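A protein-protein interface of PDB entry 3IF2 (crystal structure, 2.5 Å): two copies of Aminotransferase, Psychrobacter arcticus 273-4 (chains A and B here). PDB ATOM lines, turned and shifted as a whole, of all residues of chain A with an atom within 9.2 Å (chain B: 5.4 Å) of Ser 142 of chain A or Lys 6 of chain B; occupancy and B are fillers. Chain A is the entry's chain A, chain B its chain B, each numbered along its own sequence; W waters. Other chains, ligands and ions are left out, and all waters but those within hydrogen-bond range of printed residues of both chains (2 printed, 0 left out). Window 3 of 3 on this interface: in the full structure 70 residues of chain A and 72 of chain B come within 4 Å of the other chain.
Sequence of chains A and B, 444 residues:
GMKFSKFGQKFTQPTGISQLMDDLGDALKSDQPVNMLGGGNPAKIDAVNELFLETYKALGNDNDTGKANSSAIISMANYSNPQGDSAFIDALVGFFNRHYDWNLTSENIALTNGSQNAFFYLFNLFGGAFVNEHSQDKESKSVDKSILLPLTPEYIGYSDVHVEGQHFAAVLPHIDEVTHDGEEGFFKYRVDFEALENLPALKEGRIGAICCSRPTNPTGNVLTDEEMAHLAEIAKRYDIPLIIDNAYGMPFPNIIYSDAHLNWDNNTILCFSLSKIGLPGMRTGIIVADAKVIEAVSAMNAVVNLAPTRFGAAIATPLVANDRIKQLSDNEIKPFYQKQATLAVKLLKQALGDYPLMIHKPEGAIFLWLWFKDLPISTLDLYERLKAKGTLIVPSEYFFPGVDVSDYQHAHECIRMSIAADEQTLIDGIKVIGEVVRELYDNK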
ATOM      1  N   ASN A 124     -30.121  -1.499   1.089  1.00  0.00           N
ATOM      2  CA  ASN A 124     -29.489  -1.680  -0.227  1.00  0.00           C
ATOM      3  C   ASN A 124     -28.830  -3.056  -0.378  1.00  0.00           C
ATOM      4  O   ASN A 124     -28.621  -3.516  -1.498  1.00  0.00           O
ATOM      5  CB  ASN A 124     -28.509  -0.540  -0.517  1.00  0.00           C
ATOM      6  CG  ASN A 124     -29.221   0.727  -0.907  1.00  0.00           C
ATOM      7  OD1 ASN A 124     -29.850   0.785  -1.985  1.00  0.00           O
ATOM      8  ND2 ASN A 124     -29.144   1.743  -0.060  1.00  0.00           N
ATOM      9  N   LEU A 125     -28.502  -3.703   0.737  1.00  0.00           N
ATOM     10  CA  LEU A 125     -27.926  -5.057   0.729  1.00  0.00           C
ATOM     11  C   LEU A 125     -28.997  -6.096   0.407  1.00  0.00           C
ATOM     12  O   LEU A 125     -28.710  -7.070  -0.274  1.00  0.00           O
ATOM     13  CB  LEU A 125     -27.275  -5.380   2.085  1.00  0.00           C
ATOM     14  CG  LEU A 125     -26.497  -6.686   2.274  1.00  0.00           C
ATOM     15  CD1 LEU A 125     -25.241  -6.705   1.404  1.00  0.00           C
ATOM     16  CD2 LEU A 125     -26.141  -6.897   3.767  1.00  0.00           C
ATOM     17  N   PHE A 126     -30.222  -5.881   0.897  1.00  0.00           N
ATOM     18  CA  PHE A 126     -31.329  -6.812   0.733  1.00  0.00           C
ATOM     19  C   PHE A 126     -32.512  -6.280  -0.069  1.00  0.00           C
ATOM     20  O   PHE A 126     -33.533  -6.924  -0.117  1.00  0.00           O
ATOM     21  CB  PHE A 126     -31.807  -7.238   2.122  1.00  0.00           C
ATOM     22  CG  PHE A 126     -30.796  -8.017   2.884  1.00  0.00           C
ATOM     23  CD1 PHE A 126     -30.436  -9.299   2.452  1.00  0.00           C
ATOM     24  CD2 PHE A 126     -30.219  -7.500   4.061  1.00  0.00           C
ATOM     25  CE1 PHE A 126     -29.494 -10.063   3.148  1.00  0.00           C
ATOM     26  CE2 PHE A 126     -29.266  -8.249   4.785  1.00  0.00           C
ATOM     27  CZ  PHE A 126     -28.895  -9.534   4.324  1.00  0.00           C
ATOM     28  N   GLY A 127     -32.374  -5.118  -0.698  1.00  0.00           N
ATOM     29  CA  GLY A 127     -33.456  -4.514  -1.470  1.00  0.00           C
ATOM     30  C   GLY A 127     -32.920  -3.866  -2.730  1.00  0.00           C
ATOM     31  O   GLY A 127     -31.751  -3.467  -2.781  1.00  0.00           O
ATOM     32  N   GLY A 128     -33.808  -3.728  -3.719  1.00  0.00           N
ATOM     33  CA  GLY A 128     -33.466  -3.203  -5.039  1.00  0.00           C
ATOM     34  C   GLY A 128     -33.281  -4.346  -6.014  1.00  0.00           C
ATOM     35  O   GLY A 128     -33.834  -5.426  -5.811  1.00  0.00           O
ATOM     36  N   ALA A 129     -32.486  -4.119  -7.054  1.00  0.00           N
ATOM     37  CA  ALA A 129     -32.308  -5.109  -8.126  1.00  0.00           C
ATOM     38  C   ALA A 129     -31.501  -6.338  -7.685  1.00  0.00           C
ATOM     39  O   ALA A 129     -30.413  -6.189  -7.111  1.00  0.00           O
ATOM     40  CB  ALA A 129     -31.654  -4.459  -9.334  1.00  0.00           C
ATOM     41  N   PHE A 130     -32.068  -7.528  -7.936  1.00  0.00           N
ATOM     42  CA  PHE A 130     -31.450  -8.841  -7.697  1.00  0.00           C
ATOM     43  C   PHE A 130     -31.304  -9.604  -9.021  1.00  0.00           C
ATOM     44  O   PHE A 130     -32.089  -9.391  -9.965  1.00  0.00           O
ATOM     45  CB  PHE A 130     -32.326  -9.732  -6.805  1.00  0.00           C
ATOM     46  CG  PHE A 130     -32.181  -9.499  -5.320  1.00  0.00           C
ATOM     47  CD1 PHE A 130     -32.600  -8.313  -4.748  1.00  0.00           C
ATOM     48  CD2 PHE A 130     -31.722 -10.522  -4.480  1.00  0.00           C
ATOM     49  CE1 PHE A 130     -32.520  -8.111  -3.365  1.00  0.00           C
ATOM     50  CE2 PHE A 130     -31.643 -10.342  -3.097  1.00  0.00           C
ATOM     51  CZ  PHE A 130     -32.038  -9.132  -2.532  1.00  0.00           C
ATOM     52  N   VAL A 131     -30.344 -10.534  -9.053  1.00  0.00           N
ATOM     53  CA  VAL A 131     -30.156 -11.429 -10.191  1.00  0.00           C
ATOM     54  C   VAL A 131     -31.353 -12.397 -10.116  1.00  0.00           C
ATOM     55  O   VAL A 131     -31.673 -12.918  -9.043  1.00  0.00           O
ATOM     56  CB  VAL A 131     -28.778 -12.175 -10.191  1.00  0.00           C
ATOM     57  CG1 VAL A 131     -28.649 -13.070 -11.433  1.00  0.00           C
ATOM     58  CG2 VAL A 131     -27.626 -11.175 -10.174  1.00  0.00           C
ATOM     59  N   ASN A 132     -32.028 -12.570 -11.256  1.00  0.00           N
ATOM     60  CA  ASN A 132     -33.243 -13.404 -11.389  1.00  0.00           C
ATOM     61  C   ASN A 132     -32.866 -14.896 -11.421  1.00  0.00           C
ATOM     62  O   ASN A 132     -31.739 -15.245 -11.790  1.00  0.00           O
ATOM     63  CB  ASN A 132     -33.994 -12.960 -12.670  1.00  0.00           C
ATOM     64  CG  ASN A 132     -35.383 -13.603 -12.850  1.00  0.00           C
ATOM     65  OD1 ASN A 132     -35.942 -14.235 -11.947  1.00  0.00           O
ATOM     66  ND2 ASN A 132     -35.943 -13.420 -14.044  1.00  0.00           N
ATOM     67  N   GLU A 133     -33.812 -15.769 -11.064  1.00  0.00           N
ATOM     68  CA  GLU A 133     -33.555 -17.225 -10.971  1.00  0.00           C
ATOM     69  C   GLU A 133     -34.836 -18.065 -10.882  1.00  0.00           C
ATOM     70  O   GLU A 133     -35.218 -18.727 -11.842  1.00  0.00           O
ATOM     71  CB  GLU A 133     -32.656 -17.484  -9.743  1.00  0.00           C
ATOM     72  CG  GLU A 133     -33.121 -16.721  -8.475  1.00  0.00           C
ATOM     73  CD  GLU A 133     -32.271 -16.968  -7.243  1.00  0.00           C
ATOM     74  OE1 GLU A 133     -32.721 -16.541  -6.148  1.00  0.00           O
ATOM     75  OE2 GLU A 133     -31.168 -17.561  -7.352  1.00  0.00           O
ATOM     76  N   LYS A 141     -34.259 -11.023 -16.874  1.00  0.00           N
ATOM     77  CA  LYS A 141     -32.874 -11.310 -16.492  1.00  0.00           C
ATOM     78  C   LYS A 141     -32.513 -10.833 -15.063  1.00  0.00           C
ATOM     79  O   LYS A 141     -31.549 -11.341 -14.479  1.00  0.00           O
ATOM     80  CB  LYS A 141     -31.884 -10.731 -17.520  1.00  0.00           C
ATOM     81  N   SER A 142     -33.247  -9.845 -14.531  1.00  0.00           N
ATOM     82  CA  SER A 142     -33.095  -9.351 -13.135  1.00  0.00           C
ATOM     83  C   SER A 142     -34.490  -9.017 -12.530  1.00  0.00           C
ATOM     84  O   SER A 142     -35.469  -8.879 -13.276  1.00  0.00           O
ATOM     85  CB  SER A 142     -32.152  -8.146 -13.074  1.00  0.00           C
ATOM     86  OG  SER A 142     -32.702  -7.027 -13.740  1.00  0.00           O
ATOM     87  N   VAL A 143     -34.581  -8.884 -11.205  1.00  0.00           N
ATOM     88  CA  VAL A 143     -35.876  -8.647 -10.537  1.00  0.00           C
ATOM     89  C   VAL A 143     -35.722  -7.771  -9.301  1.00  0.00           C
ATOM     90  O   VAL A 143     -34.792  -7.965  -8.539  1.00  0.00           O
ATOM     91  CB  VAL A 143     -36.554 -10.005 -10.153  1.00  0.00           C
ATOM     92  CG1 VAL A 143     -35.625 -10.877  -9.321  1.00  0.00           C
ATOM     93  CG2 VAL A 143     -37.893  -9.796  -9.434  1.00  0.00           C
ATOM     94  N   ASP A 144     -36.628  -6.806  -9.120  1.00  0.00           N
ATOM     95  CA  ASP A 144     -36.627  -5.930  -7.933  1.00  0.00           C
ATOM     96  C   ASP A 144     -37.224  -6.637  -6.718  1.00  0.00           C
ATOM     97  O   ASP A 144     -38.214  -7.357  -6.840  1.00  0.00           O
ATOM     98  CB  ASP A 144     -37.418  -4.623  -8.177  1.00  0.00           C
ATOM     99  CG  ASP A 144     -36.644  -3.590  -8.984  1.00  0.00           C
ATOM    100  OD1 ASP A 144     -35.428  -3.766  -9.247  1.00  0.00           O
ATOM    101  OD2 ASP A 144     -37.263  -2.563  -9.325  1.00  0.00           O
ATOM    102  N   LYS A 145     -36.595  -6.450  -5.562  1.00  0.00           N
ATOM    103  CA  LYS A 145     -37.111  -6.964  -4.298  1.00  0.00           C
ATOM    104  C   LYS A 145     -37.253  -5.814  -3.307  1.00  0.00           C
ATOM    105  O   LYS A 145     -36.524  -4.826  -3.381  1.00  0.00           O
ATOM    106  CB  LYS A 145     -36.243  -8.075  -3.720  1.00  0.00           C
ATOM    107  CG  LYS A 145     -36.083  -9.263  -4.629  1.00  0.00           C
ATOM    108  CD  LYS A 145     -35.647 -10.507  -3.877  1.00  0.00           C
ATOM    109  CE  LYS A 145     -35.427 -11.641  -4.853  1.00  0.00           C
ATOM    110  NZ  LYS A 145     -35.226 -12.939  -4.185  1.00  0.00           N
ATOM    111  N   GLU A 164     -31.429   3.291  -6.032  1.00  0.00           N
ATOM    112  CA  GLU A 164     -32.250   3.471  -7.247  1.00  0.00           C
ATOM    113  C   GLU A 164     -33.709   3.178  -6.915  1.00  0.00           C
ATOM    114  O   GLU A 164     -34.009   2.124  -6.395  1.00  0.00           O
ATOM    115  CB  GLU A 164     -31.762   2.581  -8.417  1.00  0.00           C
ATOM    116  CG  GLU A 164     -32.687   2.664  -9.690  1.00  0.00           C
ATOM    117  CD  GLU A 164     -32.018   2.319 -11.058  1.00  0.00           C
ATOM    118  OE1 GLU A 164     -30.816   1.988 -11.118  1.00  0.00           O
ATOM    119  OE2 GLU A 164     -32.716   2.403 -12.103  1.00  0.00           O
ATOM    120  N   ARG A 206     -40.262 -12.036  -4.078  1.00  0.00           N
ATOM    121  CA  ARG A 206     -39.846 -10.655  -4.374  1.00  0.00           C
ATOM    122  C   ARG A 206     -39.662  -9.776  -3.119  1.00  0.00           C
ATOM    123  O   ARG A 206     -39.715  -8.537  -3.202  1.00  0.00           O
ATOM    124  CB  ARG A 206     -40.845 -10.021  -5.363  1.00  0.00           C
ATOM    125  CG  ARG A 206     -40.916 -10.759  -6.704  1.00  0.00           C
ATOM    126  CD  ARG A 206     -41.798 -10.045  -7.739  1.00  0.00           C
ATOM    127  NE  ARG A 206     -43.206  -9.986  -7.357  1.00  0.00           N
ATOM    128  CZ  ARG A 206     -43.815  -8.909  -6.868  1.00  0.00           C
ATOM    129  NH1 ARG A 206     -43.149  -7.772  -6.701  1.00  0.00           N
ATOM    130  NH2 ARG A 206     -45.104  -8.972  -6.556  1.00  0.00           N
ATOM    131  N   MET A 300     -18.400  -2.810   3.067  1.00  0.00           N
ATOM    132  CA  MET A 300     -19.056  -1.535   2.745  1.00  0.00           C
ATOM    133  C   MET A 300     -18.443  -0.328   3.522  1.00  0.00           C
ATOM    134  O   MET A 300     -18.249   0.746   2.937  1.00  0.00           O
ATOM    135  CB  MET A 300     -20.568  -1.626   2.979  1.00  0.00           C
ATOM    136  CG  MET A 300     -21.290  -2.424   1.921  1.00  0.00           C
ATOM    137  SD  MET A 300     -23.178  -2.545   2.338  1.00  0.00           S
ATOM    138  CE  MET A 300     -23.786  -3.689   0.877  1.00  0.00           C
ATOM    139  N   PHE B   4     -28.179 -11.775  -1.335  1.00  0.00           N
ATOM    140  CA  PHE B   4     -27.897 -10.335  -1.424  1.00  0.00           C
ATOM    141  C   PHE B   4     -28.313  -9.794  -2.780  1.00  0.00           C
ATOM    142  O   PHE B   4     -28.443 -10.534  -3.749  1.00  0.00           O
ATOM    143  CB  PHE B   4     -26.404 -10.005  -1.254  1.00  0.00           C
ATOM    144  CG  PHE B   4     -25.795 -10.371   0.084  1.00  0.00           C
ATOM    145  CD1 PHE B   4     -26.551 -10.462   1.269  1.00  0.00           C
ATOM    146  CD2 PHE B   4     -24.402 -10.492   0.182  1.00  0.00           C
ATOM    147  CE1 PHE B   4     -25.936 -10.769   2.503  1.00  0.00           C
ATOM    148  CE2 PHE B   4     -23.779 -10.779   1.417  1.00  0.00           C
ATOM    149  CZ  PHE B   4     -24.548 -10.917   2.575  1.00  0.00           C
ATOM    150  N   SER B   5     -28.483  -8.479  -2.848  1.00  0.00           N
ATOM    151  CA  SER B   5     -28.817  -7.797  -4.094  1.00  0.00           C
ATOM    152  C   SER B   5     -27.572  -7.684  -4.990  1.00  0.00           C
ATOM    153  O   SER B   5     -26.468  -8.072  -4.592  1.00  0.00           O
ATOM    154  CB  SER B   5     -29.329  -6.400  -3.765  1.00  0.00           C
ATOM    155  OG  SER B   5     -28.308  -5.639  -3.145  1.00  0.00           O
ATOM    156  N   LYS B   6     -27.748  -7.144  -6.196  1.00  0.00           N
ATOM    157  CA  LYS B   6     -26.614  -6.853  -7.095  1.00  0.00           C
ATOM    158  C   LYS B   6     -25.679  -5.861  -6.409  1.00  0.00           C
ATOM    159  O   LYS B   6     -24.445  -5.983  -6.514  1.00  0.00           O
ATOM    160  CB  LYS B   6     -27.071  -6.278  -8.441  1.00  0.00           C
ATOM    161  CG  LYS B   6     -27.744  -7.268  -9.421  1.00  0.00           C
ATOM    162  CD  LYS B   6     -28.280  -6.502 -10.652  1.00  0.00           C
ATOM    163  CE  LYS B   6     -28.644  -7.408 -11.828  1.00  0.00           C
ATOM    164  NZ  LYS B   6     -27.420  -7.961 -12.496  1.00  0.00           N
ATOM    165  N   PHE B   7     -26.282  -4.891  -5.711  1.00  0.00           N
ATOM    166  CA  PHE B   7     -25.554  -3.917  -4.903  1.00  0.00           C
ATOM    167  C   PHE B   7     -24.671  -4.655  -3.867  1.00  0.00           C
ATOM    168  O   PHE B   7     -23.470  -4.429  -3.800  1.00  0.00           O
ATOM    169  CB  PHE B   7     -26.545  -2.946  -4.224  1.00  0.00           C
ATOM    170  CG  PHE B   7     -25.891  -1.876  -3.418  1.00  0.00           C
ATOM    171  CD1 PHE B   7     -25.608  -0.629  -3.989  1.00  0.00           C
ATOM    172  CD2 PHE B   7     -25.528  -2.110  -2.088  1.00  0.00           C
ATOM    173  CE1 PHE B   7     -24.965   0.368  -3.227  1.00  0.00           C
ATOM    174  CE2 PHE B   7     -24.887  -1.125  -1.328  1.00  0.00           C
ATOM    175  CZ  PHE B   7     -24.614   0.118  -1.891  1.00  0.00           C
ATOM    176  N   GLY B   8     -25.274  -5.562  -3.105  1.00  0.00           N
ATOM    177  CA  GLY B   8     -24.557  -6.372  -2.112  1.00  0.00           C
ATOM    178  C   GLY B   8     -23.467  -7.267  -2.688  1.00  0.00           C
ATOM    179  O   GLY B   8     -22.404  -7.394  -2.096  1.00  0.00           O
ATOM    180  N   GLN B   9     -23.744  -7.892  -3.831  1.00  0.00           N
ATOM    181  CA  GLN B   9     -22.747  -8.727  -4.528  1.00  0.00           C
ATOM    182  C   GLN B   9     -21.491  -7.939  -4.939  1.00  0.00           C
ATOM    183  O   GLN B   9     -20.402  -8.489  -4.884  1.00  0.00           O
ATOM    184  CB  GLN B   9     -23.363  -9.442  -5.725  1.00  0.00           C
ATOM    185  CG  GLN B   9     -24.268 -10.552  -5.321  1.00  0.00           C
ATOM    186  CD  GLN B   9     -25.015 -11.140  -6.499  1.00  0.00           C
ATOM    187  OE1 GLN B   9     -25.834 -10.478  -7.143  1.00  0.00           O
ATOM    188  NE2 GLN B   9     -24.751 -12.399  -6.775  1.00  0.00           N
ATOM    189  N   LYS B  10     -21.650  -6.664  -5.318  1.00  0.00           N
ATOM    190  CA  LYS B  10     -20.514  -5.785  -5.656  1.00  0.00           C
ATOM    191  C   LYS B  10     -19.562  -5.528  -4.458  1.00  0.00           C
ATOM    192  O   LYS B  10     -18.346  -5.515  -4.637  1.00  0.00           O
ATOM    193  CB  LYS B  10     -20.982  -4.445  -6.281  1.00  0.00           C
ATOM    194  CG  LYS B  10     -19.844  -3.381  -6.414  1.00  0.00           C
ATOM    195  CD  LYS B  10     -20.200  -2.185  -7.274  1.00  0.00           C
ATOM    196  CE  LYS B  10     -18.988  -1.279  -7.451  1.00  0.00           C
ATOM    197  NZ  LYS B  10     -18.430  -0.724  -6.192  1.00  0.00           N
ATOM    198  N   GLU B 164     -22.602   1.432  -8.973  1.00  0.00           N
ATOM    199  CA  GLU B 164     -22.722   0.388 -10.025  1.00  0.00           C
ATOM    200  C   GLU B 164     -21.577   0.471 -11.026  1.00  0.00           C
ATOM    201  O   GLU B 164     -21.337   1.535 -11.603  1.00  0.00           O
ATOM    202  CB  GLU B 164     -24.065   0.438 -10.788  1.00  0.00           C
ATOM    203  CG  GLU B 164     -24.227  -0.781 -11.753  1.00  0.00           C
ATOM    204  CD  GLU B 164     -25.627  -0.963 -12.349  1.00  0.00           C
ATOM    205  OE1 GLU B 164     -26.360   0.035 -12.513  1.00  0.00           O
ATOM    206  OE2 GLU B 164     -25.982  -2.122 -12.691  1.00  0.00           O
HETATM  207  O   HOH W   1     -28.702 -10.408  -6.881  1.00  0.00           O
HETATM  208  O   HOH W   2     -28.901  -3.663  -6.395  1.00  0.00           O
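Ser 142 of chain A touches one residue of chain B. Lys 6 of chain B touches three residues of chain A. Ser 5 of chain B touches just these residues of chain A: Asn 124 (2.7 Å), Leu 125 (2.9 Å), Gly 127 (3.9 Å), Ala 129 (3.5 Å) and Phe 130 (3.6 Å). Printed residues of chain B within 4 Å of Met 300 of chain A: Phe 7. Printed residues of chain A within 4 Å of Gln 9 of chain B: Val 131. The nearest residue of chain A that does not touch Lys 6 of chain B is Phe 130 of chain A (4.3 Å). The nearest printed residue of chain B that does not touch Phe 130 of chain A is Lys 6 of chain B (4.3 Å).
Position printed for both chains: 164. Of the 15 pairs that touch across the chains among the printed residues, none has its exchanged pair printed and touching as well.
N of Phe 7 of chain B lies close to OG of Ser 5 of chain B (3.4 Å). The backbone NH (N) of Phe 130 of chain A lies within hydrogen-bond range of the backbone carbonyl oxygen (O) of Val 143 of chain A, 2.8 Å away. OG of Ser 5 of chain B is in hydrogen-bond range of N of Gly 8 of chain B, at 3.0 Å.
Water W1 lies within hydrogen-bond range of N of Val 131 of chain A (2.7 Å), OE1 of Gln 9 of chain B (2.9 Å), O of Phe 4 of chain B (3.1 Å) and N of Lys 6 of chain B (3.5 Å). Water W2 lies within hydrogen-bond range of N of Phe 7 of chain B (3.0 Å) and O of Ala 129 of chain A (3.0 Å).
Of the 18 printed residues of chain A, 9 touch a printed residue of chain B. Among the printed residues, 15 pairs touch across the chains.
OG of Ser 5 of chain B sits at hydrogen-bond distance from O of Asn 124 of chain A, 2.7 Å away. The backbone carbonyl oxygen of Leu 125 of chain A sits at hydrogen-bond distance from the backbone NH of Ser 5 of chain B (2.9 Å). The backbone carbonyl oxygen (O) of Ala 129 of chain A lies within hydrogen-bond range of the backbone NH (N) of Lys 6 of chain B, 3.0 Å away.
Asn 124 of chain A touches Phe 7 of chain B (O to CD2, 3.4 Å). Phe 4 of chain B touches Leu 125 of chain A. CD1 of Leu 125 of chain A touches CA of Gly 8 of chain B, at 3.6 Å. Phe 126 of chain A touches Phe 4 of chain B. Gly 127 of chain A touches Ser 5 of chain B. Ala 129 of chain A touches Ser 5 of chain B (O to CB, 3.5 Å). Phe 130 of chain A touches Phe 4 of chain B. OE1 of Gln 9 of chain B touches CG2 of Val 131 of chain A, 3.6 Å away. CE of Lys 6 of chain B touches CB of Ser 142 of chain A, at 3.8 Å. Phe 7 of chain B touches Met 300 of chain A.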
